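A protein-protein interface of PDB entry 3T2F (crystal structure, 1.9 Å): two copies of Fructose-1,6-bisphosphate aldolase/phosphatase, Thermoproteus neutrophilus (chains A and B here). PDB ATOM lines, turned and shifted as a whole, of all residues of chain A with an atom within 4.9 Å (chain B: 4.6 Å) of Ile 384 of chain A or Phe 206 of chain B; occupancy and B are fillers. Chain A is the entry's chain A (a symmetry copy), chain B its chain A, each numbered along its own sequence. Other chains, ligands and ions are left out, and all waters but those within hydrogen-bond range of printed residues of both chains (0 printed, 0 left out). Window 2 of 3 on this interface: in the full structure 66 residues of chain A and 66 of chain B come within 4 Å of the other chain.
The backbone NH (N) of Ile 167 of chain B is in hydrogen-bond range of the backbone carbonyl oxygen (O) of Phe 206 of chain B, at 2.8 Å. O of Lys 204 of chain B is in hydrogen-bond range of N of Glu 169 of chain B, at 2.8 Å.
Among the printed residues, pairs that only touch across the chains: Tyr 376 of chain A with Leu 180 of chain B, Val 388 of chain A with Gly 211 of chain B, Val 387 of chain A with Ile 167 of chain B, Val 388 of chain A with Arg 208 of chain B, Arg 380 of chain A with Lys 204 of chain B, Ile 384 of chain A with Phe 206 of chain B, Val 388 of chain A with Ile 167 of chain B, Ile 384 of chain A with Leu 180 of chain B and Val 387 of chain A with Leu 180 of chain B.
No position is printed for both chains.
The side-chain carboxylate (OE1) of Glu 169 of chain B lies within salt-bridge range of the guanidinium group (NH2) of Arg 380 of chain A (2.8 Å). OH of Tyr 376 of chain A lies within hydrogen-bond range of OE2 of Glu 169 of chain B, at 2.8 Å.
Printed residues of chain A that touch a printed residue of chain B: Tyr 376, Arg 380, Ile 384, Val 387 and Val 388. Along chain A the printed residues that touch a printed residue of chain B span positions 376 to 388. Printed residues of chain B that touch a printed residue of chain A: Ile 167, Glu 169, Leu 180, Lys 204, Phe 206, Arg 208 and Gly 211. Hydrophobic or aromatic side chains of chain B within 4 Å of the printed part of chain A: Ile 167, Leu 180 and Phe 206. Among the printed residues, 11 pairs touch across the chains. Among the printed residues, Asp or Glu carboxylates within 4 Å of a Lys or Arg side-chain nitrogen of the other chain: Arg 380 of chain A with Glu 169 of chain B.
Of the printed residues of chain B, Ile 384 of chain A touches Leu 180 and Phe 206. Of the printed residues of chain A, Phe 206 of chain B touches Ile 384. Printed residues of chain A within 4 Å of Ile 167 of chain B: Val 387 (3.6 Å) and Val 388 (3.9 Å). Printed residues of chain B within 4 Å of Val 388 of chain A: Ile 167 (3.9 Å), Arg 208 (3.6 Å) and Gly 211 (3.5 Å). The nearest printed residue of chain B that does not touch Ile 384 of chain A is Gly 211 of chain B (4.02 Å). The nearest printed residue of chain A that does not touch Phe 206 of chain B is Arg 380 of chain A (4.02 Å). The nearest printed residue of chain A that does not touch Leu 180 of chain B is Tyr 383 of chain A (4.01 Å).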
ATOM      1  N   TYR A 376      -7.805  10.699  -6.055  1.00  0.00           N
ATOM      2  CA  TYR A 376      -7.940  10.888  -7.514  1.00  0.00           C
ATOM      3  C   TYR A 376      -8.782  12.089  -7.872  1.00  0.00           C
ATOM      4  O   TYR A 376      -8.347  12.885  -8.685  1.00  0.00           O
ATOM      5  CB  TYR A 376      -8.484   9.650  -8.256  1.00  0.00           C
ATOM      6  CG  TYR A 376      -8.646   9.904  -9.749  1.00  0.00           C
ATOM      7  CD1 TYR A 376      -9.875  10.366 -10.278  1.00  0.00           C
ATOM      8  CD2 TYR A 376      -7.570   9.739 -10.608  1.00  0.00           C
ATOM      9  CE1 TYR A 376      -9.999  10.602 -11.722  1.00  0.00           C
ATOM     10  CE2 TYR A 376      -7.677   9.974 -12.004  1.00  0.00           C
ATOM     11  CZ  TYR A 376      -8.890  10.402 -12.528  1.00  0.00           C
ATOM     12  OH  TYR A 376      -8.969  10.604 -13.890  1.00  0.00           O
ATOM     13  N   ARG A 380      -7.590  15.000 -10.506  1.00  0.00           N
ATOM     14  CA  ARG A 380      -7.963  14.446 -11.848  1.00  0.00           C
ATOM     15  C   ARG A 380      -7.218  15.169 -12.995  1.00  0.00           C
ATOM     16  O   ARG A 380      -6.511  14.543 -13.839  1.00  0.00           O
ATOM     17  CB  ARG A 380      -9.497  14.502 -12.057  1.00  0.00           C
ATOM     18  CG  ARG A 380      -9.925  14.153 -13.518  1.00  0.00           C
ATOM     19  CD  ARG A 380     -11.390  14.297 -13.671  1.00  0.00           C
ATOM     20  NE  ARG A 380     -12.118  13.143 -13.169  1.00  0.00           N
ATOM     21  CZ  ARG A 380     -13.012  13.183 -12.199  1.00  0.00           C
ATOM     22  NH1 ARG A 380     -13.296  14.329 -11.571  1.00  0.00           N
ATOM     23  NH2 ARG A 380     -13.636  12.077 -11.825  1.00  0.00           N
ATOM     24  N   LYS A 381      -7.370  16.507 -12.982  1.00  0.00           N
ATOM     25  CA  LYS A 381      -6.692  17.389 -13.946  1.00  0.00           C
ATOM     26  C   LYS A 381      -5.212  17.126 -14.059  1.00  0.00           C
ATOM     27  O   LYS A 381      -4.678  17.101 -15.205  1.00  0.00           O
ATOM     28  CB  LYS A 381      -6.991  18.873 -13.742  1.00  0.00           C
ATOM     29  CG  LYS A 381      -8.029  19.427 -14.735  1.00  0.00           C
ATOM     30  CD  LYS A 381      -9.500  19.519 -14.145  1.00  0.00           C
ATOM     31  CE  LYS A 381      -9.955  20.966 -13.707  1.00  0.00           C
ATOM     32  NZ  LYS A 381     -10.499  20.980 -12.259  1.00  0.00           N
ATOM     33  N   LYS A 382      -4.536  16.862 -12.932  1.00  0.00           N
ATOM     34  CA  LYS A 382      -3.056  16.681 -13.049  1.00  0.00           C
ATOM     35  C   LYS A 382      -2.814  15.375 -13.751  1.00  0.00           C
ATOM     36  O   LYS A 382      -1.948  15.261 -14.645  1.00  0.00           O
ATOM     37  CB  LYS A 382      -2.310  16.616 -11.674  1.00  0.00           C
ATOM     38  CG  LYS A 382      -2.289  17.876 -10.820  1.00  0.00           C
ATOM     39  CD  LYS A 382      -3.026  17.686  -9.446  1.00  0.00           C
ATOM     40  CE  LYS A 382      -4.431  18.410  -9.340  1.00  0.00           C
ATOM     41  NZ  LYS A 382      -5.287  18.335 -10.609  1.00  0.00           N
ATOM     42  N   TYR A 383      -3.577  14.381 -13.290  1.00  0.00           N
ATOM     43  CA  TYR A 383      -3.457  13.025 -13.798  1.00  0.00           C
ATOM     44  C   TYR A 383      -3.702  12.949 -15.272  1.00  0.00           C
ATOM     45  O   TYR A 383      -2.914  12.315 -15.988  1.00  0.00           O
ATOM     46  CB  TYR A 383      -4.378  12.080 -13.030  1.00  0.00           C
ATOM     47  CG  TYR A 383      -3.864  11.782 -11.655  1.00  0.00           C
ATOM     48  CD1 TYR A 383      -2.568  11.286 -11.467  1.00  0.00           C
ATOM     49  CD2 TYR A 383      -4.653  12.038 -10.527  1.00  0.00           C
ATOM     50  CE1 TYR A 383      -2.082  11.027 -10.180  1.00  0.00           C
ATOM     51  CE2 TYR A 383      -4.184  11.771  -9.222  1.00  0.00           C
ATOM     52  CZ  TYR A 383      -2.894  11.268  -9.069  1.00  0.00           C
ATOM     53  OH  TYR A 383      -2.455  10.992  -7.800  1.00  0.00           O
ATOM     54  N   ILE A 384      -4.779  13.607 -15.736  1.00  0.00           N
ATOM     55  CA  ILE A 384      -5.069  13.648 -17.196  1.00  0.00           C
ATOM     56  C   ILE A 384      -4.000  14.408 -17.980  1.00  0.00           C
ATOM     57  O   ILE A 384      -3.544  13.921 -19.028  1.00  0.00           O
ATOM     58  CB  ILE A 384      -6.463  14.238 -17.543  1.00  0.00           C
ATOM     59  CG1 ILE A 384      -7.602  13.501 -16.811  1.00  0.00           C
ATOM     60  CG2 ILE A 384      -6.620  14.284 -19.056  1.00  0.00           C
ATOM     61  CD1 ILE A 384      -7.677  12.004 -17.061  1.00  0.00           C
ATOM     62  N   GLU A 385      -3.567  15.592 -17.503  1.00  0.00           N
ATOM     63  CA  GLU A 385      -2.511  16.325 -18.232  1.00  0.00           C
ATOM     64  C   GLU A 385      -1.217  15.501 -18.321  1.00  0.00           C
ATOM     65  O   GLU A 385      -0.565  15.436 -19.373  1.00  0.00           O
ATOM     66  CB  GLU A 385      -2.221  17.641 -17.559  1.00  0.00           C
ATOM     67  CG  GLU A 385      -3.251  18.699 -17.826  1.00  0.00           C
ATOM     68  CD  GLU A 385      -2.933  20.002 -17.052  1.00  0.00           C
ATOM     69  OE1 GLU A 385      -1.710  20.357 -16.980  1.00  0.00           O
ATOM     70  OE2 GLU A 385      -3.890  20.644 -16.508  1.00  0.00           O
ATOM     71  N   ALA A 386      -0.895  14.818 -17.229  1.00  0.00           N
ATOM     72  CA  ALA A 386       0.212  13.873 -17.202  1.00  0.00           C
ATOM     73  C   ALA A 386       0.075  12.843 -18.297  1.00  0.00           C
ATOM     74  O   ALA A 386       1.014  12.667 -19.082  1.00  0.00           O
ATOM     75  CB  ALA A 386       0.320  13.199 -15.849  1.00  0.00           C
ATOM     76  N   VAL A 387      -1.095  12.167 -18.374  1.00  0.00           N
ATOM     77  CA  VAL A 387      -1.288  11.174 -19.431  1.00  0.00           C
ATOM     78  C   VAL A 387      -1.190  11.809 -20.793  1.00  0.00           C
ATOM     79  O   VAL A 387      -0.645  11.194 -21.675  1.00  0.00           O
ATOM     80  CB  VAL A 387      -2.644  10.395 -19.323  1.00  0.00           C
ATOM     81  CG1 VAL A 387      -2.793   9.460 -20.537  1.00  0.00           C
ATOM     82  CG2 VAL A 387      -2.764   9.644 -17.977  1.00  0.00           C
ATOM     83  N   VAL A 388      -1.707  13.037 -20.965  1.00  0.00           N
ATOM     84  CA  VAL A 388      -1.690  13.716 -22.268  1.00  0.00           C
ATOM     85  C   VAL A 388      -0.268  14.142 -22.747  1.00  0.00           C
ATOM     86  O   VAL A 388       0.109  13.937 -23.928  1.00  0.00           O
ATOM     87  CB  VAL A 388      -2.630  14.969 -22.270  1.00  0.00           C
ATOM     88  CG1 VAL A 388      -2.428  15.831 -23.545  1.00  0.00           C
ATOM     89  CG2 VAL A 388      -4.122  14.564 -22.074  1.00  0.00           C
ATOM     90  N   PHE B 166      -8.108   7.635 -26.987  1.00  0.00           N
ATOM     91  CA  PHE B 166      -8.829   8.206 -25.864  1.00  0.00           C
ATOM     92  C   PHE B 166      -8.352   7.667 -24.557  1.00  0.00           C
ATOM     93  O   PHE B 166      -7.732   6.558 -24.517  1.00  0.00           O
ATOM     94  CB  PHE B 166     -10.361   7.876 -26.019  1.00  0.00           C
ATOM     95  CG  PHE B 166     -10.984   8.672 -27.137  1.00  0.00           C
ATOM     96  CD1 PHE B 166     -11.563   9.964 -26.862  1.00  0.00           C
ATOM     97  CD2 PHE B 166     -10.898   8.218 -28.449  1.00  0.00           C
ATOM     98  CE1 PHE B 166     -12.018  10.796 -27.965  1.00  0.00           C
ATOM     99  CE2 PHE B 166     -11.429   9.017 -29.524  1.00  0.00           C
ATOM    100  CZ  PHE B 166     -11.975  10.293 -29.266  1.00  0.00           C
ATOM    101  N   ILE B 167      -8.679   8.412 -23.494  1.00  0.00           N
ATOM    102  CA  ILE B 167      -8.320   8.025 -22.143  1.00  0.00           C
ATOM    103  C   ILE B 167      -9.584   7.666 -21.400  1.00  0.00           C
ATOM    104  O   ILE B 167     -10.513   8.460 -21.339  1.00  0.00           O
ATOM    105  CB  ILE B 167      -7.588   9.236 -21.377  1.00  0.00           C
ATOM    106  CG1 ILE B 167      -6.334   9.600 -22.200  1.00  0.00           C
ATOM    107  CG2 ILE B 167      -7.258   8.755 -19.912  1.00  0.00           C
ATOM    108  CD1 ILE B 167      -5.740  11.031 -21.847  1.00  0.00           C
ATOM    109  N   GLU B 169     -11.403   6.712 -17.850  1.00  0.00           N
ATOM    110  CA  GLU B 169     -11.302   6.709 -16.411  1.00  0.00           C
ATOM    111  C   GLU B 169     -12.274   5.701 -15.905  1.00  0.00           C
ATOM    112  O   GLU B 169     -13.473   5.847 -16.047  1.00  0.00           O
ATOM    113  CB  GLU B 169     -11.650   8.114 -15.891  1.00  0.00           C
ATOM    114  CG  GLU B 169     -11.769   8.167 -14.345  1.00  0.00           C
ATOM    115  CD  GLU B 169     -12.224   9.537 -13.880  1.00  0.00           C
ATOM    116  OE1 GLU B 169     -13.133   9.611 -13.019  1.00  0.00           O
ATOM    117  OE2 GLU B 169     -11.701  10.539 -14.448  1.00  0.00           O
ATOM    118  N   LEU B 180      -6.691   4.571 -15.104  1.00  0.00           N
ATOM    119  CA  LEU B 180      -6.656   5.349 -16.284  1.00  0.00           C
ATOM    120  C   LEU B 180      -6.047   4.555 -17.400  1.00  0.00           C
ATOM    121  O   LEU B 180      -4.827   4.145 -17.379  1.00  0.00           O
ATOM    122  CB  LEU B 180      -5.842   6.588 -16.057  1.00  0.00           C
ATOM    123  CG  LEU B 180      -6.486   7.679 -15.252  1.00  0.00           C
ATOM    124  CD1 LEU B 180      -5.410   8.839 -15.146  1.00  0.00           C
ATOM    125  CD2 LEU B 180      -7.766   8.214 -15.972  1.00  0.00           C
ATOM    126  N   LYS B 204     -15.494   8.416 -16.964  1.00  0.00           N
ATOM    127  CA  LYS B 204     -15.293   9.502 -17.855  1.00  0.00           C
ATOM    128  C   LYS B 204     -14.415   9.045 -19.005  1.00  0.00           C
ATOM    129  O   LYS B 204     -13.602   8.093 -18.851  1.00  0.00           O
ATOM    130  CB  LYS B 204     -14.573  10.691 -17.048  1.00  0.00           C
ATOM    131  CG  LYS B 204     -15.539  11.276 -15.950  1.00  0.00           C
ATOM    132  CD  LYS B 204     -15.098  12.598 -15.166  1.00  0.00           C
ATOM    133  CE  LYS B 204     -16.313  13.233 -14.321  1.00  0.00           C
ATOM    134  NZ  LYS B 204     -17.042  14.352 -15.204  1.00  0.00           N
ATOM    135  N   VAL B 205     -14.500   9.799 -20.124  1.00  0.00           N
ATOM    136  CA  VAL B 205     -13.595   9.571 -21.197  1.00  0.00           C
ATOM    137  C   VAL B 205     -13.040  10.944 -21.675  1.00  0.00           C
ATOM    138  O   VAL B 205     -13.785  11.925 -21.661  1.00  0.00           O
ATOM    139  CB  VAL B 205     -14.361   8.940 -22.423  1.00  0.00           C
ATOM    140  CG1 VAL B 205     -13.357   8.693 -23.584  1.00  0.00           C
ATOM    141  CG2 VAL B 205     -15.036   7.612 -21.978  1.00  0.00           C
ATOM    142  N   PHE B 206     -11.739  10.970 -21.975  1.00  0.00           N
ATOM    143  CA  PHE B 206     -11.076  12.184 -22.431  1.00  0.00           C
ATOM    144  C   PHE B 206     -10.386  11.950 -23.732  1.00  0.00           C
ATOM    145  O   PHE B 206      -9.881  10.903 -24.006  1.00  0.00           O
ATOM    146  CB  PHE B 206     -10.030  12.662 -21.360  1.00  0.00           C
ATOM    147  CG  PHE B 206     -10.638  12.886 -20.076  1.00  0.00           C
ATOM    148  CD1 PHE B 206     -11.171  14.111 -19.778  1.00  0.00           C
ATOM    149  CD2 PHE B 206     -10.668  11.883 -19.129  1.00  0.00           C
ATOM    150  CE1 PHE B 206     -11.767  14.370 -18.504  1.00  0.00           C
ATOM    151  CE2 PHE B 206     -11.288  12.106 -17.842  1.00  0.00           C
ATOM    152  CZ  PHE B 206     -11.835  13.347 -17.550  1.00  0.00           C
ATOM    153  N   ARG B 207     -10.384  12.960 -24.580  1.00  0.00           N
ATOM    154  CA  ARG B 207      -9.621  12.916 -25.776  1.00  0.00           C
ATOM    155  C   ARG B 207      -8.103  12.884 -25.460  1.00  0.00           C
ATOM    156  O   ARG B 207      -7.641  13.645 -24.587  1.00  0.00           O
ATOM    157  CB  ARG B 207     -10.067  14.076 -26.714  1.00  0.00           C
ATOM    158  CG  ARG B 207      -9.086  14.076 -27.767  1.00  0.00           C
ATOM    159  CD  ARG B 207      -9.701  14.260 -29.019  1.00  0.00           C
ATOM    160  NE  ARG B 207     -10.006  15.618 -29.293  1.00  0.00           N
ATOM    161  CZ  ARG B 207      -9.503  16.243 -30.359  1.00  0.00           C
ATOM    162  NH1 ARG B 207      -8.658  15.603 -31.167  1.00  0.00           N
ATOM    163  NH2 ARG B 207      -9.875  17.495 -30.635  1.00  0.00           N
ATOM    164  N   ARG B 208      -7.343  11.967 -26.062  1.00  0.00           N
ATOM    165  CA  ARG B 208      -5.906  11.860 -25.739  1.00  0.00           C
ATOM    166  C   ARG B 208      -5.081  13.034 -26.326  1.00  0.00           C
ATOM    167  O   ARG B 208      -4.105  13.456 -25.710  1.00  0.00           O
ATOM    168  CB  ARG B 208      -5.292  10.559 -26.223  1.00  0.00           C
ATOM    169  CG  ARG B 208      -4.335  10.008 -25.204  1.00  0.00           C
ATOM    170  CD  ARG B 208      -3.022   9.581 -25.812  1.00  0.00           C
ATOM    171  NE  ARG B 208      -3.358   8.252 -26.253  1.00  0.00           N
ATOM    172  CZ  ARG B 208      -2.609   7.180 -26.225  1.00  0.00           C
ATOM    173  NH1 ARG B 208      -1.331   7.201 -25.823  1.00  0.00           N
ATOM    174  NH2 ARG B 208      -3.181   6.068 -26.698  1.00  0.00           N
ATOM    175  N   GLY B 211      -6.685  16.108 -23.907  1.00  0.00           N
ATOM    176  CA  GLY B 211      -7.339  15.959 -22.637  1.00  0.00           C
ATOM    177  C   GLY B 211      -8.778  16.476 -22.643  1.00  0.00           C
ATOM    178  O   GLY B 211      -9.371  16.556 -21.596  1.00  0.00           O
ATOM    179  N   ALA B 212      -9.335  16.884 -23.759  1.00  0.00           N
ATOM    180  CA  ALA B 212     -10.720  17.460 -23.681  1.00  0.00           C
ATOM    181  C   ALA B 212     -11.736  16.402 -23.124  1.00  0.00           C
ATOM    182  O   ALA B 212     -11.592  15.235 -23.460  1.00  0.00           O
ATOM    183  CB  ALA B 212     -11.190  17.865 -25.019  1.00  0.00           C
ATOM    184  N   PRO B 213     -12.733  16.820 -22.346  1.00  0.00           N
ATOM    185  CA  PRO B 213     -13.655  15.786 -21.836  1.00  0.00           C
ATOM    186  C   PRO B 213     -14.575  15.354 -22.993  1.00  0.00           C
ATOM    187  O   PRO B 213     -15.013  16.189 -23.755  1.00  0.00           O
ATOM    188  CB  PRO B 213     -14.469  16.473 -20.729  1.00  0.00           C
ATOM    189  CG  PRO B 213     -14.136  18.022 -20.858  1.00  0.00           C
ATOM    190  CD  PRO B 213     -12.857  18.118 -21.630  1.00  0.00           C
ATOM    191  N   ALA B 214     -14.821  14.029 -23.119  1.00  0.00           N
ATOM    192  CA  ALA B 214     -15.591  13.533 -24.263  1.00  0.00           C
ATOM    193  C   ALA B 214     -16.905  12.896 -23.759  1.00  0.00           C
ATOM    194  O   ALA B 214     -17.897  13.039 -24.431  1.00  0.00           O
ATOM    195  CB  ALA B 214     -14.772  12.504 -25.062  1.00  0.00           C
